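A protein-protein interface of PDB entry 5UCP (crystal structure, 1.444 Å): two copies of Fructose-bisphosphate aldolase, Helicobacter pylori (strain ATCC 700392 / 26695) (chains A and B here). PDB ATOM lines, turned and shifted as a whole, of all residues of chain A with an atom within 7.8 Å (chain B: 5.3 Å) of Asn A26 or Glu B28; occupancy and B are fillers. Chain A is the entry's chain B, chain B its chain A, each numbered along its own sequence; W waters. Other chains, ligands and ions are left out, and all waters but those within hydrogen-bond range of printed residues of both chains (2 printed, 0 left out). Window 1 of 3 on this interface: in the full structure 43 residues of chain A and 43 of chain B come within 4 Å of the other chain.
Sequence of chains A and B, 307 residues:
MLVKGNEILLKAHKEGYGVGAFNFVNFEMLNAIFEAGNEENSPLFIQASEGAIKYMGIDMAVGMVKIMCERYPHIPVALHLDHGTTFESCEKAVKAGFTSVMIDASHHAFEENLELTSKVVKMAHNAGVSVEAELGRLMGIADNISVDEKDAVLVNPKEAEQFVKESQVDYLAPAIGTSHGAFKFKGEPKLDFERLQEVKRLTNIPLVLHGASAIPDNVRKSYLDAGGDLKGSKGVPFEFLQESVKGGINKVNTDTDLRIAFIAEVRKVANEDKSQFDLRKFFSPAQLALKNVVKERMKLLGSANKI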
ATOM      1  N   ASN A  23      22.148  16.185  -3.013  1.00  0.00           N
ATOM      2  CA  ASN A  23      23.148  17.221  -3.186  1.00  0.00           C
ATOM      3  C   ASN A  23      22.648  18.301  -4.136  1.00  0.00           C
ATOM      4  O   ASN A  23      21.836  18.047  -5.027  1.00  0.00           O
ATOM      5  CB  ASN A  23      24.430  16.616  -3.746  1.00  0.00           C
ATOM      6  CG  ASN A  23      25.192  15.831  -2.721  1.00  0.00           C
ATOM      7  OD1 ASN A  23      24.862  14.685  -2.414  1.00  0.00           O
ATOM      8  ND2 ASN A  23      26.232  16.437  -2.188  1.00  0.00           N
ATOM      9  N   PHE A  24      23.158  19.514  -3.944  1.00  0.00           N
ATOM     10  CA  PHE A  24      22.875  20.607  -4.869  1.00  0.00           C
ATOM     11  C   PHE A  24      24.136  21.432  -5.050  1.00  0.00           C
ATOM     12  O   PHE A  24      25.015  21.454  -4.186  1.00  0.00           O
ATOM     13  CB  PHE A  24      21.716  21.509  -4.414  1.00  0.00           C
ATOM     14  CG  PHE A  24      22.060  22.489  -3.307  1.00  0.00           C
ATOM     15  CD1 PHE A  24      22.245  22.044  -2.008  1.00  0.00           C
ATOM     16  CD2 PHE A  24      22.116  23.859  -3.558  1.00  0.00           C
ATOM     17  CE1 PHE A  24      22.536  22.936  -0.979  1.00  0.00           C
ATOM     18  CE2 PHE A  24      22.400  24.758  -2.531  1.00  0.00           C
ATOM     19  CZ  PHE A  24      22.613  24.293  -1.244  1.00  0.00           C
ATOM     20  N   VAL A  25      24.216  22.112  -6.196  1.00  0.00           N
ATOM     21  CA  VAL A  25      25.323  23.026  -6.464  1.00  0.00           C
ATOM     22  C   VAL A  25      24.831  24.396  -6.928  1.00  0.00           C
ATOM     23  O   VAL A  25      25.643  25.311  -7.084  1.00  0.00           O
ATOM     24  CB  VAL A  25      26.326  22.460  -7.489  1.00  0.00           C
ATOM     25  CG1 VAL A  25      26.809  21.088  -7.074  1.00  0.00           C
ATOM     26  CG2 VAL A  25      25.737  22.433  -8.894  1.00  0.00           C
ATOM     27  N   ASN A  26      23.531  24.562  -7.169  1.00  0.00           N
ATOM     28  CA  ASN A  26      23.022  25.848  -7.634  1.00  0.00           C
ATOM     29  C   ASN A  26      21.512  25.925  -7.403  1.00  0.00           C
ATOM     30  O   ASN A  26      20.908  25.047  -6.776  1.00  0.00           O
ATOM     31  CB  ASN A  26      23.430  26.108  -9.088  1.00  0.00           C
ATOM     32  CG  ASN A  26      22.741  25.193 -10.077  1.00  0.00           C
ATOM     33  OD1 ASN A  26      21.800  24.457  -9.745  1.00  0.00           O
ATOM     34  ND2 ASN A  26      23.214  25.234 -11.321  1.00  0.00           N
ATOM     35  N   PHE A  27      20.896  26.992  -7.926  1.00  0.00           N
ATOM     36  CA  PHE A  27      19.474  27.237  -7.695  1.00  0.00           C
ATOM     37  C   PHE A  27      18.604  26.191  -8.380  1.00  0.00           C
ATOM     38  O   PHE A  27      17.637  25.702  -7.793  1.00  0.00           O
ATOM     39  CB  PHE A  27      19.068  28.643  -8.157  1.00  0.00           C
ATOM     40  CG  PHE A  27      17.577  28.807  -8.329  1.00  0.00           C
ATOM     41  CD1 PHE A  27      16.757  28.877  -7.214  1.00  0.00           C
ATOM     42  CD2 PHE A  27      16.994  28.818  -9.582  1.00  0.00           C
ATOM     43  CE1 PHE A  27      15.391  28.995  -7.341  1.00  0.00           C
ATOM     44  CE2 PHE A  27      15.624  28.934  -9.716  1.00  0.00           C
ATOM     45  CZ  PHE A  27      14.821  29.011  -8.583  1.00  0.00           C
ATOM     46  N   GLU A  28      18.934  25.821  -9.618  1.00  0.00           N
ATOM     47  CA  GLU A  28      18.094  24.887 -10.359  1.00  0.00           C
ATOM     48  C   GLU A  28      17.961  23.553  -9.637  1.00  0.00           C
ATOM     49  O   GLU A  28      16.860  22.995  -9.531  1.00  0.00           O
ATOM     50  CB  GLU A  28      18.680  24.675 -11.740  1.00  0.00           C
ATOM     51  CG  GLU A  28      18.282  25.760 -12.703  1.00  0.00           C
ATOM     52  CD  GLU A  28      19.088  27.048 -12.604  1.00  0.00           C
ATOM     53  OE1 GLU A  28      20.121  27.092 -11.892  1.00  0.00           O
ATOM     54  OE2 GLU A  28      18.678  28.011 -13.287  1.00  0.00           O
ATOM     55  N   MET A  29      19.078  23.010  -9.158  1.00  0.00           N
ATOM     56  CA  MET A  29      19.011  21.744  -8.440  1.00  0.00           C
ATOM     57  C   MET A  29      18.194  21.904  -7.169  1.00  0.00           C
ATOM     58  O   MET A  29      17.341  21.066  -6.850  1.00  0.00           O
ATOM     59  CB  MET A  29      20.424  21.263  -8.095  1.00  0.00           C
ATOM     60  CG  MET A  29      21.280  20.864  -9.284  1.00  0.00           C
ATOM     61  SD  MET A  29      22.827  20.092  -8.794  1.00  0.00           S
ATOM     62  CE  MET A  29      22.271  18.484  -8.270  1.00  0.00           C
ATOM     63  N   LEU A  30      18.436  22.982  -6.436  1.00  0.00           N
ATOM     64  CA  LEU A  30      17.756  23.178  -5.165  1.00  0.00           C
ATOM     65  C   LEU A  30      16.257  23.332  -5.356  1.00  0.00           C
ATOM     66  O   LEU A  30      15.463  22.754  -4.607  1.00  0.00           O
ATOM     67  CB  LEU A  30      18.347  24.380  -4.449  1.00  0.00           C
ATOM     68  CG  LEU A  30      17.890  24.640  -3.027  1.00  0.00           C
ATOM     69  CD1 LEU A  30      18.358  23.528  -2.126  1.00  0.00           C
ATOM     70  CD2 LEU A  30      18.432  25.961  -2.544  1.00  0.00           C
ATOM     71  N   ASN A  31      15.844  24.112  -6.349  1.00  0.00           N
ATOM     72  CA  ASN A  31      14.420  24.319  -6.551  1.00  0.00           C
ATOM     73  C   ASN A  31      13.715  23.008  -6.882  1.00  0.00           C
ATOM     74  O   ASN A  31      12.626  22.738  -6.370  1.00  0.00           O
ATOM     75  CB  ASN A  31      14.215  25.353  -7.655  1.00  0.00           C
ATOM     76  CG  ASN A  31      12.760  25.786  -7.786  1.00  0.00           C
ATOM     77  OD1 ASN A  31      12.118  26.171  -6.802  1.00  0.00           O
ATOM     78  ND2 ASN A  31      12.226  25.683  -8.989  1.00  0.00           N
ATOM     79  N   ALA A  32      14.322  22.187  -7.743  1.00  0.00           N
ATOM     80  CA  ALA A  32      13.726  20.919  -8.139  1.00  0.00           C
ATOM     81  C   ALA A  32      13.612  19.958  -6.962  1.00  0.00           C
ATOM     82  O   ALA A  32      12.608  19.247  -6.828  1.00  0.00           O
ATOM     83  CB  ALA A  32      14.556  20.315  -9.266  1.00  0.00           C
ATOM     84  N   ILE A  33      14.633  19.916  -6.105  1.00  0.00           N
ATOM     85  CA  ILE A  33      14.571  19.076  -4.910  1.00  0.00           C
ATOM     86  C   ILE A  33      13.414  19.506  -4.019  1.00  0.00           C
ATOM     87  O   ILE A  33      12.639  18.675  -3.543  1.00  0.00           O
ATOM     88  CB  ILE A  33      15.913  19.118  -4.168  1.00  0.00           C
ATOM     89  CG1 ILE A  33      16.999  18.444  -5.000  1.00  0.00           C
ATOM     90  CG2 ILE A  33      15.797  18.434  -2.809  1.00  0.00           C
ATOM     91  CD1 ILE A  33      18.413  18.788  -4.501  1.00  0.00           C
ATOM     92  N   ALA A  52      30.920  22.023  -3.683  1.00  0.00           N
ATOM     93  CA  ALA A  52      29.744  22.834  -3.966  1.00  0.00           C
ATOM     94  C   ALA A  52      29.781  24.140  -3.185  1.00  0.00           C
ATOM     95  O   ALA A  52      29.427  25.203  -3.711  1.00  0.00           O
ATOM     96  CB  ALA A  52      28.493  22.046  -3.609  1.00  0.00           C
ATOM     97  N   TYR A  55      32.029  26.526  -4.806  1.00  0.00           N
ATOM     98  CA  TYR A  55      31.432  27.028  -6.041  1.00  0.00           C
ATOM     99  C   TYR A  55      30.388  28.109  -5.761  1.00  0.00           C
ATOM    100  O   TYR A  55      30.394  29.173  -6.407  1.00  0.00           O
ATOM    101  CB  TYR A  55      30.838  25.839  -6.794  1.00  0.00           C
ATOM    102  CG  TYR A  55      30.099  26.182  -8.063  1.00  0.00           C
ATOM    103  CD1 TYR A  55      30.778  26.333  -9.264  1.00  0.00           C
ATOM    104  CD2 TYR A  55      28.720  26.328  -8.064  1.00  0.00           C
ATOM    105  CE1 TYR A  55      30.100  26.636 -10.420  1.00  0.00           C
ATOM    106  CE2 TYR A  55      28.037  26.632  -9.220  1.00  0.00           C
ATOM    107  CZ  TYR A  55      28.731  26.776 -10.390  1.00  0.00           C
ATOM    108  OH  TYR A  55      28.051  27.083 -11.545  1.00  0.00           O
ATOM    109  N   MET A  56      29.477  27.866  -4.800  1.00  0.00           N
ATOM    110  CA  MET A  56      28.414  28.818  -4.489  1.00  0.00           C
ATOM    111  C   MET A  56      28.881  29.911  -3.542  1.00  0.00           C
ATOM    112  O   MET A  56      28.378  31.036  -3.607  1.00  0.00           O
ATOM    113  CB  MET A  56      27.236  28.110  -3.811  1.00  0.00           C
ATOM    114  CG  MET A  56      26.369  27.290  -4.742  1.00  0.00           C
ATOM    115  SD  MET A  56      25.080  26.408  -3.828  1.00  0.00           S
ATOM    116  CE  MET A  56      26.036  25.054  -3.156  1.00  0.00           C
ATOM    117  N   MET A  60      25.960  31.849   0.142  1.00  0.00           N
ATOM    118  CA  MET A  60      24.891  31.638  -0.830  1.00  0.00           C
ATOM    119  C   MET A  60      24.251  30.267  -0.663  1.00  0.00           C
ATOM    120  O   MET A  60      23.033  30.116  -0.821  1.00  0.00           O
ATOM    121  CB  MET A  60      25.439  31.793  -2.247  1.00  0.00           C
ATOM    122  CG  MET A  60      24.363  31.667  -3.332  1.00  0.00           C
ATOM    123  SD  MET A  60      23.098  32.958  -3.318  1.00  0.00           S
ATOM    124  CE  MET A  60      24.053  34.362  -3.879  1.00  0.00           C
ATOM    125  N   MET A  64      20.327  30.508   0.040  1.00  0.00           N
ATOM    126  CA  MET A  64      19.311  29.975  -0.857  1.00  0.00           C
ATOM    127  C   MET A  64      18.435  28.954  -0.144  1.00  0.00           C
ATOM    128  O   MET A  64      17.216  28.932  -0.333  1.00  0.00           O
ATOM    129  CB  MET A  64      19.943  29.351  -2.104  1.00  0.00           C
ATOM    130  CG  MET A  64      20.543  30.345  -3.079  1.00  0.00           C
ATOM    131  SD  MET A  64      20.926  29.627  -4.695  1.00  0.00           S
ATOM    132  CE  MET A  64      21.938  28.240  -4.248  1.00  0.00           C
ATOM    133  N   PHE A 262      19.585  15.813 -14.983  1.00  0.00           N
ATOM    134  CA  PHE A 262      19.612  17.235 -15.309  1.00  0.00           C
ATOM    135  C   PHE A 262      20.367  17.473 -16.611  1.00  0.00           C
ATOM    136  O   PHE A 262      19.835  18.070 -17.552  1.00  0.00           O
ATOM    137  CB  PHE A 262      20.269  17.977 -14.149  1.00  0.00           C
ATOM    138  CG  PHE A 262      20.200  19.465 -14.239  1.00  0.00           C
ATOM    139  CD1 PHE A 262      19.231  20.164 -13.538  1.00  0.00           C
ATOM    140  CD2 PHE A 262      21.123  20.168 -14.992  1.00  0.00           C
ATOM    141  CE1 PHE A 262      19.167  21.541 -13.607  1.00  0.00           C
ATOM    142  CE2 PHE A 262      21.073  21.555 -15.057  1.00  0.00           C
ATOM    143  CZ  PHE A 262      20.093  22.236 -14.359  1.00  0.00           C
ATOM    144  N   LEU A 279      18.723  30.556 -21.196  1.00  0.00           N
ATOM    145  CA  LEU A 279      19.098  29.607 -20.149  1.00  0.00           C
ATOM    146  C   LEU A 279      17.883  28.863 -19.616  1.00  0.00           C
ATOM    147  O   LEU A 279      17.971  27.671 -19.290  1.00  0.00           O
ATOM    148  CB  LEU A 279      19.823  30.333 -19.015  1.00  0.00           C
ATOM    149  CG  LEU A 279      21.337  30.566 -19.148  1.00  0.00           C
ATOM    150  CD1 LEU A 279      21.683  31.534 -20.244  1.00  0.00           C
ATOM    151  CD2 LEU A 279      21.926  31.062 -17.836  1.00  0.00           C
ATOM    152  N   PHE A 283      17.164  24.888 -18.695  1.00  0.00           N
ATOM    153  CA  PHE A 283      17.138  24.443 -17.306  1.00  0.00           C
ATOM    154  C   PHE A 283      15.745  24.152 -16.767  1.00  0.00           C
ATOM    155  O   PHE A 283      15.635  23.482 -15.733  1.00  0.00           O
ATOM    156  CB  PHE A 283      17.868  25.447 -16.412  1.00  0.00           C
ATOM    157  CG  PHE A 283      19.288  25.694 -16.838  1.00  0.00           C
ATOM    158  CD1 PHE A 283      20.035  24.674 -17.416  1.00  0.00           C
ATOM    159  CD2 PHE A 283      19.869  26.939 -16.694  1.00  0.00           C
ATOM    160  CE1 PHE A 283      21.333  24.891 -17.830  1.00  0.00           C
ATOM    161  CE2 PHE A 283      21.165  27.163 -17.105  1.00  0.00           C
ATOM    162  CZ  PHE A 283      21.902  26.136 -17.676  1.00  0.00           C
ATOM    163  N   GLN A 287      15.349  20.827 -14.657  1.00  0.00           N
ATOM    164  CA  GLN A 287      14.733  20.809 -13.338  1.00  0.00           C
ATOM    165  C   GLN A 287      13.645  19.746 -13.255  1.00  0.00           C
ATOM    166  O   GLN A 287      13.550  19.019 -12.262  1.00  0.00           O
ATOM    167  CB  GLN A 287      14.117  22.172 -13.037  1.00  0.00           C
ATOM    168  CG  GLN A 287      15.089  23.251 -12.571  1.00  0.00           C
ATOM    169  CD  GLN A 287      14.367  24.463 -12.054  1.00  0.00           C
ATOM    170  OE1 GLN A 287      13.621  24.388 -11.080  1.00  0.00           O
ATOM    171  NE2 GLN A 287      14.558  25.595 -12.723  1.00  0.00           N
ATOM    172  N   LEU A 290      15.124  16.298 -12.986  1.00  0.00           N
ATOM    173  CA  LEU A 290      15.706  16.084 -11.665  1.00  0.00           C
ATOM    174  C   LEU A 290      14.606  15.907 -10.622  1.00  0.00           C
ATOM    175  O   LEU A 290      14.652  14.985  -9.798  1.00  0.00           O
ATOM    176  CB  LEU A 290      16.640  17.245 -11.322  1.00  0.00           C
ATOM    177  CG  LEU A 290      17.569  17.106 -10.121  1.00  0.00           C
ATOM    178  CD1 LEU A 290      18.729  18.098 -10.280  1.00  0.00           C
ATOM    179  CD2 LEU A 290      16.836  17.334  -8.802  1.00  0.00           C
ATOM    180  N   ASN B  26      19.520  33.323 -12.836  1.00  0.00           N
ATOM    181  CA  ASN B  26      19.907  32.326 -11.845  1.00  0.00           C
ATOM    182  C   ASN B  26      21.196  32.763 -11.156  1.00  0.00           C
ATOM    183  O   ASN B  26      21.707  33.869 -11.386  1.00  0.00           O
ATOM    184  CB  ASN B  26      19.974  30.935 -12.484  1.00  0.00           C
ATOM    185  CG  ASN B  26      21.123  30.763 -13.470  1.00  0.00           C
ATOM    186  OD1 ASN B  26      22.029  31.608 -13.608  1.00  0.00           O
ATOM    187  ND2 ASN B  26      21.096  29.626 -14.169  1.00  0.00           N
ATOM    188  N   PHE B  27      21.722  31.877 -10.305  1.00  0.00           N
ATOM    189  CA  PHE B  27      22.919  32.182  -9.529  1.00  0.00           C
ATOM    190  C   PHE B  27      24.129  32.421 -10.423  1.00  0.00           C
ATOM    191  O   PHE B  27      24.905  33.352 -10.196  1.00  0.00           O
ATOM    192  CB  PHE B  27      23.229  31.041  -8.559  1.00  0.00           C
ATOM    193  CG  PHE B  27      24.611  31.122  -7.983  1.00  0.00           C
ATOM    194  CD1 PHE B  27      24.945  32.144  -7.120  1.00  0.00           C
ATOM    195  CD2 PHE B  27      25.590  30.213  -8.346  1.00  0.00           C
ATOM    196  CE1 PHE B  27      26.212  32.262  -6.615  1.00  0.00           C
ATOM    197  CE2 PHE B  27      26.881  30.321  -7.832  1.00  0.00           C
ATOM    198  CZ  PHE B  27      27.186  31.352  -6.969  1.00  0.00           C
ATOM    199  N   GLU B  28      24.342  31.554 -11.417  1.00  0.00           N
ATOM    200  CA  GLU B  28      25.561  31.631 -12.216  1.00  0.00           C
ATOM    201  C   GLU B  28      25.686  32.979 -12.915  1.00  0.00           C
ATOM    202  O   GLU B  28      26.766  33.585 -12.919  1.00  0.00           O
ATOM    203  CB  GLU B  28      25.591  30.500 -13.237  1.00  0.00           C
ATOM    204  CG  GLU B  28      26.104  29.188 -12.681  1.00  0.00           C
ATOM    205  CD  GLU B  28      25.055  28.374 -11.952  1.00  0.00           C
ATOM    206  OE1 GLU B  28      23.860  28.751 -11.977  1.00  0.00           O
ATOM    207  OE2 GLU B  28      25.439  27.326 -11.386  1.00  0.00           O
ATOM    208  N   MET B  29      24.604  33.455 -13.530  1.00  0.00           N
ATOM    209  CA  MET B  29      24.646  34.770 -14.171  1.00  0.00           C
ATOM    210  C   MET B  29      24.952  35.854 -13.150  1.00  0.00           C
ATOM    211  O   MET B  29      25.786  36.738 -13.387  1.00  0.00           O
ATOM    212  CB  MET B  29      23.323  35.076 -14.880  1.00  0.00           C
ATOM    213  CG  MET B  29      23.032  34.163 -16.052  1.00  0.00           C
ATOM    214  SD  MET B  29      21.578  34.678 -16.969  1.00  0.00           S
ATOM    215  CE  MET B  29      22.183  36.081 -17.889  1.00  0.00           C
ATOM    216  N   LEU B  30      24.266  35.809 -12.011  1.00  0.00           N
ATOM    217  CA  LEU B  30      24.412  36.842 -11.000  1.00  0.00           C
ATOM    218  C   LEU B  30      25.831  36.883 -10.450  1.00  0.00           C
ATOM    219  O   LEU B  30      26.405  37.959 -10.261  1.00  0.00           O
ATOM    220  CB  LEU B  30      23.404  36.599  -9.890  1.00  0.00           C
ATOM    221  CG  LEU B  30      23.290  37.682  -8.844  1.00  0.00           C
ATOM    222  CD1 LEU B  30      22.794  38.964  -9.471  1.00  0.00           C
ATOM    223  CD2 LEU B  30      22.371  37.219  -7.735  1.00  0.00           C
ATOM    224  N   ASN B  31      26.400  35.716 -10.150  1.00  0.00           N
ATOM    225  CA  ASN B  31      27.754  35.686  -9.616  1.00  0.00           C
ATOM    226  C   ASN B  31      28.748  36.293 -10.594  1.00  0.00           C
ATOM    227  O   ASN B  31      29.626  37.063 -10.197  1.00  0.00           O
ATOM    228  CB  ASN B  31      28.128  34.248  -9.275  1.00  0.00           C
ATOM    229  CG  ASN B  31      29.426  34.157  -8.481  1.00  0.00           C
ATOM    230  OD1 ASN B  31      29.593  34.843  -7.465  1.00  0.00           O
ATOM    231  ND2 ASN B  31      30.362  33.343  -8.960  1.00  0.00           N
ATOM    232  N   ALA B  32      28.626  35.955 -11.877  1.00  0.00           N
ATOM    233  CA  ALA B  32      29.562  36.460 -12.875  1.00  0.00           C
ATOM    234  C   ALA B  32      29.446  37.974 -13.036  1.00  0.00           C
ATOM    235  O   ALA B  32      30.459  38.672 -13.185  1.00  0.00           O
ATOM    236  CB  ALA B  32      29.329  35.736 -14.197  1.00  0.00           C
ATOM    237  N   ILE B  33      28.224  38.505 -13.013  1.00  0.00           N
ATOM    238  CA  ILE B  33      28.036  39.953 -13.092  1.00  0.00           C
ATOM    239  C   ILE B  33      28.708  40.648 -11.910  1.00  0.00           C
ATOM    240  O   ILE B  33      29.382  41.673 -12.071  1.00  0.00           O
ATOM    241  CB  ILE B  33      26.536  40.284 -13.165  1.00  0.00           C
ATOM    242  CG1 ILE B  33      25.904  39.777 -14.473  1.00  0.00           C
ATOM    243  CG2 ILE B  33      26.306  41.788 -13.031  1.00  0.00           C
ATOM    244  CD1 ILE B  33      24.368  39.729 -14.420  1.00  0.00           C
ATOM    245  N   PHE B 262      27.543  32.695 -22.307  1.00  0.00           N
ATOM    246  CA  PHE B 262      27.332  31.622 -21.338  1.00  0.00           C
ATOM    247  C   PHE B 262      27.045  30.305 -22.043  1.00  0.00           C
ATOM    248  O   PHE B 262      27.718  29.292 -21.801  1.00  0.00           O
ATOM    249  CB  PHE B 262      26.160  32.007 -20.430  1.00  0.00           C
ATOM    250  CG  PHE B 262      25.968  31.109 -19.251  1.00  0.00           C
ATOM    251  CD1 PHE B 262      26.513  31.438 -18.016  1.00  0.00           C
ATOM    252  CD2 PHE B 262      25.219  29.956 -19.360  1.00  0.00           C
ATOM    253  CE1 PHE B 262      26.328  30.623 -16.932  1.00  0.00           C
ATOM    254  CE2 PHE B 262      25.031  29.135 -18.270  1.00  0.00           C
ATOM    255  CZ  PHE B 262      25.585  29.473 -17.057  1.00  0.00           C
ATOM    256  N   LEU B 279      27.708  19.606 -13.024  1.00  0.00           N
ATOM    257  CA  LEU B 279      27.183  20.900 -13.452  1.00  0.00           C
ATOM    258  C   LEU B 279      28.256  21.977 -13.405  1.00  0.00           C
ATOM    259  O   LEU B 279      28.253  22.893 -14.238  1.00  0.00           O
ATOM    260  CB  LEU B 279      25.988  21.311 -12.585  1.00  0.00           C
ATOM    261  CG  LEU B 279      24.616  20.777 -13.007  1.00  0.00           C
ATOM    262  CD1 LEU B 279      24.535  19.264 -12.864  1.00  0.00           C
ATOM    263  CD2 LEU B 279      23.532  21.457 -12.187  1.00  0.00           C
ATOM    264  N   PHE B 283      29.337  25.063 -15.955  1.00  0.00           N
ATOM    265  CA  PHE B 283      28.954  26.431 -15.627  1.00  0.00           C
ATOM    266  C   PHE B 283      30.092  27.296 -15.114  1.00  0.00           C
ATOM    267  O   PHE B 283      29.953  28.527 -15.122  1.00  0.00           O
ATOM    268  CB  PHE B 283      27.790  26.439 -14.638  1.00  0.00           C
ATOM    269  CG  PHE B 283      26.582  25.704 -15.144  1.00  0.00           C
ATOM    270  CD1 PHE B 283      26.285  25.686 -16.497  1.00  0.00           C
ATOM    271  CD2 PHE B 283      25.767  24.990 -14.279  1.00  0.00           C
ATOM    272  CE1 PHE B 283      25.189  25.000 -16.974  1.00  0.00           C
ATOM    273  CE2 PHE B 283      24.674  24.296 -14.757  1.00  0.00           C
ATOM    274  CZ  PHE B 283      24.389  24.300 -16.108  1.00  0.00           C
ATOM    275  N   GLN B 287      30.366  30.899 -16.630  1.00  0.00           N
ATOM    276  CA  GLN B 287      30.479  32.100 -15.817  1.00  0.00           C
ATOM    277  C   GLN B 287      31.645  32.969 -16.271  1.00  0.00           C
ATOM    278  O   GLN B 287      31.520  34.190 -16.373  1.00  0.00           O
ATOM    279  CB  GLN B 287      30.678  31.727 -14.354  1.00  0.00           C
ATOM    280  CG  GLN B 287      29.429  31.323 -13.620  1.00  0.00           C
ATOM    281  CD  GLN B 287      29.683  31.208 -12.137  1.00  0.00           C
ATOM    282  OE1 GLN B 287      30.075  32.176 -11.489  1.00  0.00           O
ATOM    283  NE2 GLN B 287      29.503  30.014 -11.602  1.00  0.00           N
HETATM  284  O   HOH W   1      21.657  28.748 -10.447  1.00  0.00           O
HETATM  285  O   HOH W   2      31.162  29.850  -9.101  1.00  0.00           O
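ND2 of Asn B26 is in hydrogen-bond range of OE2 of Glu A28.
The side-chain carboxylate (OE2) of Glu B28 lies within hydrogen-bond range of the side-chain amide nitrogen (ND2) of Asn A26, 3.1 Å away.
The side-chain carboxylate (OE2) of Glu B28 sits at hydrogen-bond distance from the side-chain hydroxyl (OH) of Tyr A55 (2.6 Å).
NE2 of Gln B287 sits at hydrogen-bond distance from OH of Tyr A55.
The backbone NH (N) of Glu B28 lies within hydrogen-bond range of the side-chain amide oxygen (OD1) of Asn B26 (3.2 Å).
N of Met B29 is in hydrogen-bond range of OD1 of Asn B26, at 3.2 Å.
The side-chain amide oxygen (OE1) of Gln B287 lies within hydrogen-bond range of the side-chain amide nitrogen (ND2) of Asn B31.
SD of Met A29 is in hydrogen-bond range of N of Val A25, 3.6 Å away.
The backbone NH (N) of Glu A28 lies within hydrogen-bond range of the side-chain amide oxygen (OD1) of Asn A26, at 3.2 Å.
N of Met A29 is in hydrogen-bond range of OD1 of Asn A26, 3.1 Å away.
Water W1 lies within hydrogen-bond range of OE1 of Glu B28 (2.7 Å), OE1 of Glu A28 (2.7 Å), N of Phe B27 (3.1 Å) and N of Phe A27 (3.2 Å).
Water W2 bridges the backbone carbonyl oxygen of Tyr A55 (2.9 Å) and the side-chain amide nitrogen of Gln B287 (3.0 Å).
Hydrophobic or aromatic side chains of chain B that line the printed part of chain A: Phe B27, Met B29, Phe B262, Leu B279 and Phe B283.
Among the printed residues, 17 pairs touch across the chains.
Among the printed residues, no Asp or Glu carboxylate lies within 4 Å of a Lys or Arg side-chain nitrogen of the other chain.
Of chain B, only Glu B28 (3.1 Å), Leu B279 (3.9 Å) and Phe B283 (3.8 Å) come within 4 Å of Asn A26.
Of the printed residues of chain B, Phe A283 touches Asn B26 (3.8 Å) and Phe B283 (3.5 Å).
Of the printed residues of chain B, Met A60 touches Phe B27 (3.8 Å).
The nearest printed residue of chain B that does not touch Met A29 is Phe B283 (7.3 Å).
Asn A26 touches Glu B28, and with the chains exchanged Glu A28 touches Asn B26.
Met A29 touches Leu B279, and with the chains exchanged Leu A279 touches Met B29.
Phe A262 touches Leu B279, and with the chains exchanged Leu A279 touches Phe B262.
Phe B283 touches its own counterpart, Phe A283.
Of the 17 pairs that touch across the chains among the printed residues, 9 have their exchanged pair printed and touching as well.
Val A25 touches Leu B279.
ND2 of Asn A26 touches CD2 of Leu B279 (3.9 Å).
Asn A26 touches Phe B283 (ND2 to CE2, 3.8 Å).
O of Tyr A55 touches CZ of Phe B27, at 3.9 Å.
CG of Met A60 touches CE1 of Phe B27 (3.8 Å).
Phe A262 touches Leu B279 (CE2 to CD2, 3.8 Å).
CD2 of Leu A279 touches SD of Met B29, 3.7 Å away.
Leu A279 touches Phe B262 (CD2 to CE2, 3.7 Å).
Phe A283 touches Asn B26.
CZ of Phe A283 touches CZ of Phe B283, at 3.5 Å.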
